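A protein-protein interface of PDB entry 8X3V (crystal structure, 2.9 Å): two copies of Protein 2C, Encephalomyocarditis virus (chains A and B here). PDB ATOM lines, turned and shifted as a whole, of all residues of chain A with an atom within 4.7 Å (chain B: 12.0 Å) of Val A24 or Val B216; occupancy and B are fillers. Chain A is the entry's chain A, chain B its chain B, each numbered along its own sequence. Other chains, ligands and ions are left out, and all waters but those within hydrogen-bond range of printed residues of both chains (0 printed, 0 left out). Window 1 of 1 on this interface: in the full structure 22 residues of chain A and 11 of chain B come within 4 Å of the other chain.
The backbone carbonyl oxygen (O) of Cys A165 is in hydrogen-bond range of the backbone NH (N) of Ala B217 (2.6 Å). The side-chain amide nitrogen of Gln A27 is in hydrogen-bond range of the backbone carbonyl oxygen of Val B212, 2.7 Å away. NE2 of Gln A37 lies within hydrogen-bond range of O of Val B216 (3.0 Å). The side-chain amide nitrogen (NE2) of Gln A37 is in hydrogen-bond range of the backbone carbonyl oxygen (O) of Ala B217 (3.1 Å). NZ of Lys A31 is in hydrogen-bond range of O of Gln B218 (2.7 Å).
Of the 16 printed residues of chain A, 9 touch a printed residue of chain B. Hydrophobic or aromatic side chains of chain A within 4 Å of the printed part of chain B: Leu A20, Val A24 and Phe A166. Of the 14 printed residues of chain B, 7 touch a printed residue of chain A.
Leu A20 touches three residues of chain B. No residue of chain B comes within 4 Å of Ser A21. No residue of chain B comes within 4 Å of Ser A22. Of the printed residues of chain B, Gln A23 touches Val B212 (3.9 Å). Of chain B, only Val B216 comes within 4 Å of Val A24. No residue of chain B comes within 4 Å of Ile A25. No residue of chain B comes within 4 Å of Ala A26. Of chain B, only Val B212 (2.7 Å) and Val B216 (3.4 Å) come within 4 Å of Gln A27. Of chain B, only Val B216 (3.8 Å) comes within 4 Å of Ala A28. Of the printed residues of chain B, Lys A31 touches Ala B217 and Gln B218. Lys B205 touches none of the printed residues of chain A. Of the printed residues of chain A, Val B208 touches Leu A20. Of the printed residues of chain A, Leu B215 touches Cys A165 and Phe A166. Val B216 touches six residues of chain A. The nearest residue of chain A that does not touch Val B216 is Lys A31 (4.3 Å).
No position is printed for both chains. Of the 18 pairs that touch across the chains among the printed residues, none has its exchanged pair printed and touching as well.
Among the printed residues, pairs that only touch across the chains: Phe A166 with Leu B215, Cys A165 with Val B216, Gln A27 with Val B216, Phe A166 with Val B216, Lys A31 with Ala B217, Gln A37 with Gln B218, Leu A20 with Val B212, Cys A165 with Leu B215, Leu A20 with Thr B211, Val A24 with Val B216, Leu A20 with Val B208, Ala A28 with Val B216 and Gln A23 with Val B212.
The backbone carbonyl oxygen (O) of Lys B207 lies within hydrogen-bond range of the side-chain hydroxyl (OG1) of Thr B211, 3.5 Å away. The side-chain amide nitrogen (NE2) of Gln A27 sits close to the side-chain amide oxygen (OE1) of Gln A37 (3.3 Å). The backbone carbonyl oxygen (O) of Ala A28 sits close to the side-chain sulfur (SG) of Cys A165 (3.8 Å).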
ATOM      1  N   LEU A  20       6.978   1.272  -9.868  1.00  0.00           N
ATOM      2  CA  LEU A  20       7.100   0.800 -11.239  1.00  0.00           C
ATOM      3  C   LEU A  20       6.208  -0.407 -11.460  1.00  0.00           C
ATOM      4  O   LEU A  20       5.399  -0.436 -12.393  1.00  0.00           O
ATOM      5  CB  LEU A  20       8.551   0.447 -11.532  1.00  0.00           C
ATOM      6  CG  LEU A  20       8.848  -0.172 -12.885  1.00  0.00           C
ATOM      7  CD1 LEU A  20       8.637   0.821 -13.995  1.00  0.00           C
ATOM      8  CD2 LEU A  20      10.284  -0.657 -12.873  1.00  0.00           C
ATOM      9  N   SER A  21       6.324  -1.404 -10.576  1.00  0.00           N
ATOM     10  CA  SER A  21       5.495  -2.594 -10.687  1.00  0.00           C
ATOM     11  C   SER A  21       4.018  -2.258 -10.593  1.00  0.00           C
ATOM     12  O   SER A  21       3.214  -2.755 -11.380  1.00  0.00           O
ATOM     13  CB  SER A  21       5.879  -3.591  -9.612  1.00  0.00           C
ATOM     14  OG  SER A  21       7.266  -3.687  -9.576  1.00  0.00           O
ATOM     15  N   SER A  22       3.636  -1.415  -9.641  1.00  0.00           N
ATOM     16  CA  SER A  22       2.228  -1.067  -9.505  1.00  0.00           C
ATOM     17  C   SER A  22       1.692  -0.534 -10.822  1.00  0.00           C
ATOM     18  O   SER A  22       0.749  -1.085 -11.388  1.00  0.00           O
ATOM     19  CB  SER A  22       2.038  -0.058  -8.379  1.00  0.00           C
ATOM     20  OG  SER A  22       2.388   1.230  -8.807  1.00  0.00           O
ATOM     21  N   GLN A  23       2.333   0.498 -11.355  1.00  0.00           N
ATOM     22  CA  GLN A  23       2.034   0.994 -12.691  1.00  0.00           C
ATOM     23  C   GLN A  23       1.998  -0.093 -13.751  1.00  0.00           C
ATOM     24  O   GLN A  23       1.031  -0.208 -14.509  1.00  0.00           O
ATOM     25  CB  GLN A  23       3.085   2.018 -13.107  1.00  0.00           C
ATOM     26  CG  GLN A  23       3.183   3.256 -12.234  1.00  0.00           C
ATOM     27  CD  GLN A  23       2.144   4.270 -12.625  1.00  0.00           C
ATOM     28  OE1 GLN A  23       1.648   4.269 -13.768  1.00  0.00           O
ATOM     29  NE2 GLN A  23       1.778   5.136 -11.676  1.00  0.00           N
ATOM     30  N   VAL A  24       3.050  -0.907 -13.835  1.00  0.00           N
ATOM     31  CA  VAL A  24       3.102  -1.868 -14.930  1.00  0.00           C
ATOM     32  C   VAL A  24       2.140  -3.028 -14.657  1.00  0.00           C
ATOM     33  O   VAL A  24       1.685  -3.687 -15.593  1.00  0.00           O
ATOM     34  CB  VAL A  24       4.542  -2.350 -15.163  1.00  0.00           C
ATOM     35  CG1 VAL A  24       4.582  -3.514 -16.146  1.00  0.00           C
ATOM     36  CG2 VAL A  24       5.344  -1.232 -15.713  1.00  0.00           C
ATOM     37  N   ILE A  25       1.775  -3.293 -13.410  1.00  0.00           N
ATOM     38  CA  ILE A  25       0.707  -4.267 -13.200  1.00  0.00           C
ATOM     39  C   ILE A  25      -0.635  -3.669 -13.618  1.00  0.00           C
ATOM     40  O   ILE A  25      -1.467  -4.344 -14.239  1.00  0.00           O
ATOM     41  CB  ILE A  25       0.697  -4.762 -11.740  1.00  0.00           C
ATOM     42  CG1 ILE A  25       1.927  -5.628 -11.459  1.00  0.00           C
ATOM     43  CG2 ILE A  25      -0.530  -5.561 -11.458  1.00  0.00           C
ATOM     44  CD1 ILE A  25       2.294  -5.655 -10.010  1.00  0.00           C
ATOM     45  N   ALA A  26      -0.864  -2.394 -13.302  1.00  0.00           N
ATOM     46  CA  ALA A  26      -2.144  -1.776 -13.629  1.00  0.00           C
ATOM     47  C   ALA A  26      -2.301  -1.626 -15.142  1.00  0.00           C
ATOM     48  O   ALA A  26      -3.347  -1.971 -15.704  1.00  0.00           O
ATOM     49  CB  ALA A  26      -2.265  -0.421 -12.929  1.00  0.00           C
ATOM     50  N   GLN A  27      -1.262  -1.120 -15.820  1.00  0.00           N
ATOM     51  CA  GLN A  27      -1.338  -0.976 -17.267  1.00  0.00           C
ATOM     52  C   GLN A  27      -1.549  -2.321 -17.946  1.00  0.00           C
ATOM     53  O   GLN A  27      -2.249  -2.399 -18.951  1.00  0.00           O
ATOM     54  CB  GLN A  27      -0.066  -0.321 -17.816  1.00  0.00           C
ATOM     55  CG  GLN A  27       0.300   0.994 -17.202  1.00  0.00           C
ATOM     56  CD  GLN A  27       1.666   1.485 -17.657  1.00  0.00           C
ATOM     57  OE1 GLN A  27       2.547   0.687 -17.991  1.00  0.00           O
ATOM     58  NE2 GLN A  27       1.848   2.797 -17.683  1.00  0.00           N
ATOM     59  N   ALA A  28      -0.954  -3.383 -17.435  1.00  0.00           N
ATOM     60  CA  ALA A  28      -0.966  -4.615 -18.204  1.00  0.00           C
ATOM     61  C   ALA A  28      -2.196  -5.462 -17.916  1.00  0.00           C
ATOM     62  O   ALA A  28      -2.684  -6.164 -18.812  1.00  0.00           O
ATOM     63  CB  ALA A  28       0.308  -5.426 -17.935  1.00  0.00           C
ATOM     64  N   LYS A  31      -4.926  -3.239 -19.727  1.00  0.00           N
ATOM     65  CA  LYS A  31      -4.813  -3.421 -21.172  1.00  0.00           C
ATOM     66  C   LYS A  31      -5.282  -4.810 -21.590  1.00  0.00           C
ATOM     67  O   LYS A  31      -5.888  -4.964 -22.656  1.00  0.00           O
ATOM     68  CB  LYS A  31      -3.378  -3.180 -21.645  1.00  0.00           C
ATOM     69  CG  LYS A  31      -3.127  -3.547 -23.095  1.00  0.00           C
ATOM     70  CD  LYS A  31      -4.026  -2.786 -24.037  1.00  0.00           C
ATOM     71  CE  LYS A  31      -3.718  -3.115 -25.481  1.00  0.00           C
ATOM     72  NZ  LYS A  31      -3.368  -1.894 -26.237  1.00  0.00           N
ATOM     73  N   GLN A  37      -4.879   0.550 -21.625  1.00  0.00           N
ATOM     74  CA  GLN A  37      -4.477   1.040 -20.327  1.00  0.00           C
ATOM     75  C   GLN A  37      -5.600   1.914 -19.795  1.00  0.00           C
ATOM     76  O   GLN A  37      -6.232   2.654 -20.550  1.00  0.00           O
ATOM     77  CB  GLN A  37      -3.180   1.827 -20.423  1.00  0.00           C
ATOM     78  CG  GLN A  37      -2.105   1.108 -21.137  1.00  0.00           C
ATOM     79  CD  GLN A  37      -0.727   1.615 -20.758  1.00  0.00           C
ATOM     80  OE1 GLN A  37      -0.576   2.522 -19.921  1.00  0.00           O
ATOM     81  NE2 GLN A  37       0.291   1.023 -21.368  1.00  0.00           N
ATOM     82  N   CYS A 165       0.308  -7.846 -24.215  1.00  0.00           N
ATOM     83  CA  CYS A 165       0.241  -6.444 -23.835  1.00  0.00           C
ATOM     84  C   CYS A 165       1.612  -5.848 -23.597  1.00  0.00           C
ATOM     85  O   CYS A 165       1.717  -4.642 -23.316  1.00  0.00           O
ATOM     86  CB  CYS A 165      -0.597  -6.278 -22.579  1.00  0.00           C
ATOM     87  SG  CYS A 165       0.083  -7.136 -21.166  1.00  0.00           S
ATOM     88  N   PHE A 166       2.654  -6.667 -23.668  1.00  0.00           N
ATOM     89  CA  PHE A 166       4.026  -6.210 -23.566  1.00  0.00           C
ATOM     90  C   PHE A 166       4.637  -6.120 -24.949  1.00  0.00           C
ATOM     91  O   PHE A 166       4.327  -6.924 -25.833  1.00  0.00           O
ATOM     92  CB  PHE A 166       4.840  -7.154 -22.688  1.00  0.00           C
ATOM     93  CG  PHE A 166       4.514  -7.043 -21.227  1.00  0.00           C
ATOM     94  CD1 PHE A 166       4.504  -5.817 -20.611  1.00  0.00           C
ATOM     95  CD2 PHE A 166       4.202  -8.168 -20.478  1.00  0.00           C
ATOM     96  CE1 PHE A 166       4.195  -5.719 -19.269  1.00  0.00           C
ATOM     97  CE2 PHE A 166       3.899  -8.070 -19.140  1.00  0.00           C
ATOM     98  CZ  PHE A 166       3.909  -6.852 -18.534  1.00  0.00           C
ATOM     99  N   PHE A 172      13.006  -7.493 -15.831  1.00  0.00           N
ATOM    100  CA  PHE A 172      11.970  -6.938 -14.987  1.00  0.00           C
ATOM    101  C   PHE A 172      10.790  -7.915 -14.919  1.00  0.00           C
ATOM    102  O   PHE A 172      10.213  -8.185 -13.854  1.00  0.00           O
ATOM    103  CB  PHE A 172      11.622  -5.577 -15.568  1.00  0.00           C
ATOM    104  CG  PHE A 172      10.485  -4.903 -14.921  1.00  0.00           C
ATOM    105  CD1 PHE A 172      10.353  -4.870 -13.553  1.00  0.00           C
ATOM    106  CD2 PHE A 172       9.558  -4.243 -15.715  1.00  0.00           C
ATOM    107  CE1 PHE A 172       9.290  -4.213 -12.987  1.00  0.00           C
ATOM    108  CE2 PHE A 172       8.504  -3.598 -15.173  1.00  0.00           C
ATOM    109  CZ  PHE A 172       8.351  -3.580 -13.806  1.00  0.00           C
ATOM    110  N   LEU A 191       6.691 -10.917 -12.183  1.00  0.00           N
ATOM    111  CA  LEU A 191       5.661  -9.913 -12.407  1.00  0.00           C
ATOM    112  C   LEU A 191       4.649 -10.424 -13.408  1.00  0.00           C
ATOM    113  O   LEU A 191       3.455 -10.119 -13.324  1.00  0.00           O
ATOM    114  CB  LEU A 191       6.280  -8.611 -12.893  1.00  0.00           C
ATOM    115  CG  LEU A 191       5.413  -7.366 -13.036  1.00  0.00           C
ATOM    116  CD1 LEU A 191       5.897  -6.301 -12.104  1.00  0.00           C
ATOM    117  CD2 LEU A 191       5.540  -6.858 -14.428  1.00  0.00           C
ATOM    118  N   ILE A 195       0.566 -10.787 -12.836  1.00  0.00           N
ATOM    119  CA  ILE A 195      -0.463 -10.303 -13.744  1.00  0.00           C
ATOM    120  C   ILE A 195      -1.442 -11.419 -14.064  1.00  0.00           C
ATOM    121  O   ILE A 195      -2.659 -11.274 -13.876  1.00  0.00           O
ATOM    122  CB  ILE A 195       0.167  -9.733 -15.024  1.00  0.00           C
ATOM    123  CG1 ILE A 195       0.690  -8.330 -14.765  1.00  0.00           C
ATOM    124  CG2 ILE A 195      -0.849  -9.701 -16.142  1.00  0.00           C
ATOM    125  CD1 ILE A 195       1.913  -8.014 -15.582  1.00  0.00           C
ATOM    126  N   LYS B 205      15.655   7.407 -12.560  1.00  0.00           N
ATOM    127  CA  LYS B 205      14.331   7.972 -12.803  1.00  0.00           C
ATOM    128  C   LYS B 205      13.962   7.935 -14.288  1.00  0.00           C
ATOM    129  O   LYS B 205      12.896   7.422 -14.654  1.00  0.00           O
ATOM    130  CB  LYS B 205      14.253   9.410 -12.280  1.00  0.00           C
ATOM    131  CG  LYS B 205      14.084   9.531 -10.774  1.00  0.00           C
ATOM    132  CD  LYS B 205      13.534  10.899 -10.389  1.00  0.00           C
ATOM    133  CE  LYS B 205      13.262  10.925  -8.894  1.00  0.00           C
ATOM    134  NZ  LYS B 205      13.396  12.282  -8.259  1.00  0.00           N
ATOM    135  N   LYS B 206      14.823   8.496 -15.155  1.00  0.00           N
ATOM    136  CA  LYS B 206      14.535   8.534 -16.589  1.00  0.00           C
ATOM    137  C   LYS B 206      14.206   7.145 -17.102  1.00  0.00           C
ATOM    138  O   LYS B 206      13.230   6.946 -17.832  1.00  0.00           O
ATOM    139  CB  LYS B 206      15.726   9.092 -17.385  1.00  0.00           C
ATOM    140  CG  LYS B 206      15.991  10.603 -17.356  1.00  0.00           C
ATOM    141  CD  LYS B 206      17.066  10.979 -18.412  1.00  0.00           C
ATOM    142  CE  LYS B 206      17.716  12.358 -18.195  1.00  0.00           C
ATOM    143  NZ  LYS B 206      17.308  13.400 -19.204  1.00  0.00           N
ATOM    144  N   LYS B 207      15.026   6.165 -16.734  1.00  0.00           N
ATOM    145  CA  LYS B 207      14.888   4.840 -17.309  1.00  0.00           C
ATOM    146  C   LYS B 207      13.599   4.178 -16.808  1.00  0.00           C
ATOM    147  O   LYS B 207      12.866   3.578 -17.591  1.00  0.00           O
ATOM    148  CB  LYS B 207      16.170   4.044 -17.012  1.00  0.00           C
ATOM    149  CG  LYS B 207      16.435   2.743 -17.817  1.00  0.00           C
ATOM    150  CD  LYS B 207      16.932   2.906 -19.279  1.00  0.00           C
ATOM    151  CE  LYS B 207      17.809   1.686 -19.775  1.00  0.00           C
ATOM    152  NZ  LYS B 207      17.174   0.347 -20.259  1.00  0.00           N
ATOM    153  N   VAL B 208      13.249   4.364 -15.539  1.00  0.00           N
ATOM    154  CA  VAL B 208      11.937   3.934 -15.069  1.00  0.00           C
ATOM    155  C   VAL B 208      10.829   4.624 -15.853  1.00  0.00           C
ATOM    156  O   VAL B 208       9.886   3.977 -16.326  1.00  0.00           O
ATOM    157  CB  VAL B 208      11.784   4.191 -13.562  1.00  0.00           C
ATOM    158  CG1 VAL B 208      10.316   4.075 -13.166  1.00  0.00           C
ATOM    159  CG2 VAL B 208      12.621   3.190 -12.780  1.00  0.00           C
ATOM    160  N   LEU B 209      10.910   5.948 -15.990  1.00  0.00           N
ATOM    161  CA  LEU B 209       9.839   6.684 -16.662  1.00  0.00           C
ATOM    162  C   LEU B 209       9.591   6.158 -18.073  1.00  0.00           C
ATOM    163  O   LEU B 209       8.436   6.046 -18.519  1.00  0.00           O
ATOM    164  CB  LEU B 209      10.169   8.173 -16.709  1.00  0.00           C
ATOM    165  CG  LEU B 209       9.132   9.038 -17.406  1.00  0.00           C
ATOM    166  CD1 LEU B 209       7.792   8.704 -16.824  1.00  0.00           C
ATOM    167  CD2 LEU B 209       9.424  10.492 -17.194  1.00  0.00           C
ATOM    168  N   THR B 210      10.671   5.856 -18.801  1.00  0.00           N
ATOM    169  CA  THR B 210      10.512   5.295 -20.132  1.00  0.00           C
ATOM    170  C   THR B 210       9.767   3.988 -20.052  1.00  0.00           C
ATOM    171  O   THR B 210       8.857   3.731 -20.848  1.00  0.00           O
ATOM    172  CB  THR B 210      11.877   5.093 -20.793  1.00  0.00           C
ATOM    173  OG1 THR B 210      12.456   6.369 -21.055  1.00  0.00           O
ATOM    174  CG2 THR B 210      11.747   4.320 -22.110  1.00  0.00           C
ATOM    175  N   THR B 211      10.129   3.152 -19.081  1.00  0.00           N
ATOM    176  CA  THR B 211       9.433   1.887 -18.932  1.00  0.00           C
ATOM    177  C   THR B 211       7.949   2.113 -18.699  1.00  0.00           C
ATOM    178  O   THR B 211       7.122   1.574 -19.426  1.00  0.00           O
ATOM    179  CB  THR B 211      10.063   1.067 -17.816  1.00  0.00           C
ATOM    180  OG1 THR B 211      11.306   0.575 -18.288  1.00  0.00           O
ATOM    181  CG2 THR B 211       9.220  -0.108 -17.521  1.00  0.00           C
ATOM    182  N   VAL B 212       7.600   2.957 -17.728  1.00  0.00           N
ATOM    183  CA  VAL B 212       6.200   3.212 -17.413  1.00  0.00           C
ATOM    184  C   VAL B 212       5.433   3.749 -18.614  1.00  0.00           C
ATOM    185  O   VAL B 212       4.221   3.529 -18.727  1.00  0.00           O
ATOM    186  CB  VAL B 212       6.106   4.164 -16.194  1.00  0.00           C
ATOM    187  CG1 VAL B 212       4.809   4.902 -16.160  1.00  0.00           C
ATOM    188  CG2 VAL B 212       6.266   3.366 -14.889  1.00  0.00           C
ATOM    189  N   GLN B 213       6.113   4.379 -19.555  1.00  0.00           N
ATOM    190  CA  GLN B 213       5.438   4.978 -20.695  1.00  0.00           C
ATOM    191  C   GLN B 213       5.426   4.090 -21.911  1.00  0.00           C
ATOM    192  O   GLN B 213       4.503   4.194 -22.719  1.00  0.00           O
ATOM    193  CB  GLN B 213       6.086   6.308 -21.080  1.00  0.00           C
ATOM    194  CG  GLN B 213       5.987   7.352 -19.984  1.00  0.00           C
ATOM    195  CD  GLN B 213       6.757   8.601 -20.322  1.00  0.00           C
ATOM    196  OE1 GLN B 213       7.709   8.565 -21.115  1.00  0.00           O
ATOM    197  NE2 GLN B 213       6.340   9.724 -19.743  1.00  0.00           N
ATOM    198  N   THR B 214       6.411   3.227 -22.059  1.00  0.00           N
ATOM    199  CA  THR B 214       6.410   2.211 -23.097  1.00  0.00           C
ATOM    200  C   THR B 214       6.211   0.826 -22.466  1.00  0.00           C
ATOM    201  O   THR B 214       5.659   0.706 -21.371  1.00  0.00           O
ATOM    202  CB  THR B 214       7.679   2.382 -23.914  1.00  0.00           C
ATOM    203  OG1 THR B 214       8.826   2.175 -23.072  1.00  0.00           O
ATOM    204  CG2 THR B 214       7.712   3.794 -24.456  1.00  0.00           C
ATOM    205  N   LEU B 215       6.613  -0.227 -23.164  1.00  0.00           N
ATOM    206  CA  LEU B 215       6.632  -1.582 -22.591  1.00  0.00           C
ATOM    207  C   LEU B 215       5.287  -2.260 -22.375  1.00  0.00           C
ATOM    208  O   LEU B 215       5.102  -3.389 -22.843  1.00  0.00           O
ATOM    209  CB  LEU B 215       7.320  -1.647 -21.222  1.00  0.00           C
ATOM    210  CG  LEU B 215       7.413  -3.110 -20.731  1.00  0.00           C
ATOM    211  CD1 LEU B 215       8.267  -3.997 -21.638  1.00  0.00           C
ATOM    212  CD2 LEU B 215       7.850  -3.254 -19.281  1.00  0.00           C
ATOM    213  N   VAL B 216       4.361  -1.635 -21.646  1.00  0.00           N
ATOM    214  CA  VAL B 216       2.971  -2.080 -21.747  1.00  0.00           C
ATOM    215  C   VAL B 216       2.389  -1.334 -22.938  1.00  0.00           C
ATOM    216  O   VAL B 216       2.551  -0.107 -23.061  1.00  0.00           O
ATOM    217  CB  VAL B 216       2.162  -1.806 -20.464  1.00  0.00           C
ATOM    218  CG1 VAL B 216       0.718  -2.286 -20.650  1.00  0.00           C
ATOM    219  CG2 VAL B 216       2.777  -2.521 -19.273  1.00  0.00           C
ATOM    220  N   ALA B 217       1.736  -2.079 -23.832  1.00  0.00           N
ATOM    221  CA  ALA B 217       1.075  -1.453 -24.963  1.00  0.00           C
ATOM    222  C   ALA B 217      -0.108  -0.636 -24.476  1.00  0.00           C
ATOM    223  O   ALA B 217      -0.737  -0.957 -23.463  1.00  0.00           O
ATOM    224  CB  ALA B 217       0.613  -2.486 -25.973  1.00  0.00           C
ATOM    225  N   GLN B 218      -0.412   0.412 -25.235  1.00  0.00           N
ATOM    226  CA  GLN B 218      -1.138   1.592 -24.754  1.00  0.00           C
ATOM    227  C   GLN B 218      -2.661   1.449 -24.639  1.00  0.00           C
ATOM    228  O   GLN B 218      -3.261   0.615 -25.305  1.00  0.00           O
ATOM    229  CB  GLN B 218      -0.799   2.767 -25.680  1.00  0.00           C
ATOM    230  CG  GLN B 218      -1.162   4.111 -25.127  1.00  0.00           C
ATOM    231  CD  GLN B 218      -0.426   4.420 -23.839  1.00  0.00           C
ATOM    232  OE1 GLN B 218       0.683   3.925 -23.612  1.00  0.00           O
ATOM    233  NE2 GLN B 218      -1.041   5.236 -22.978  1.00  0.00           N
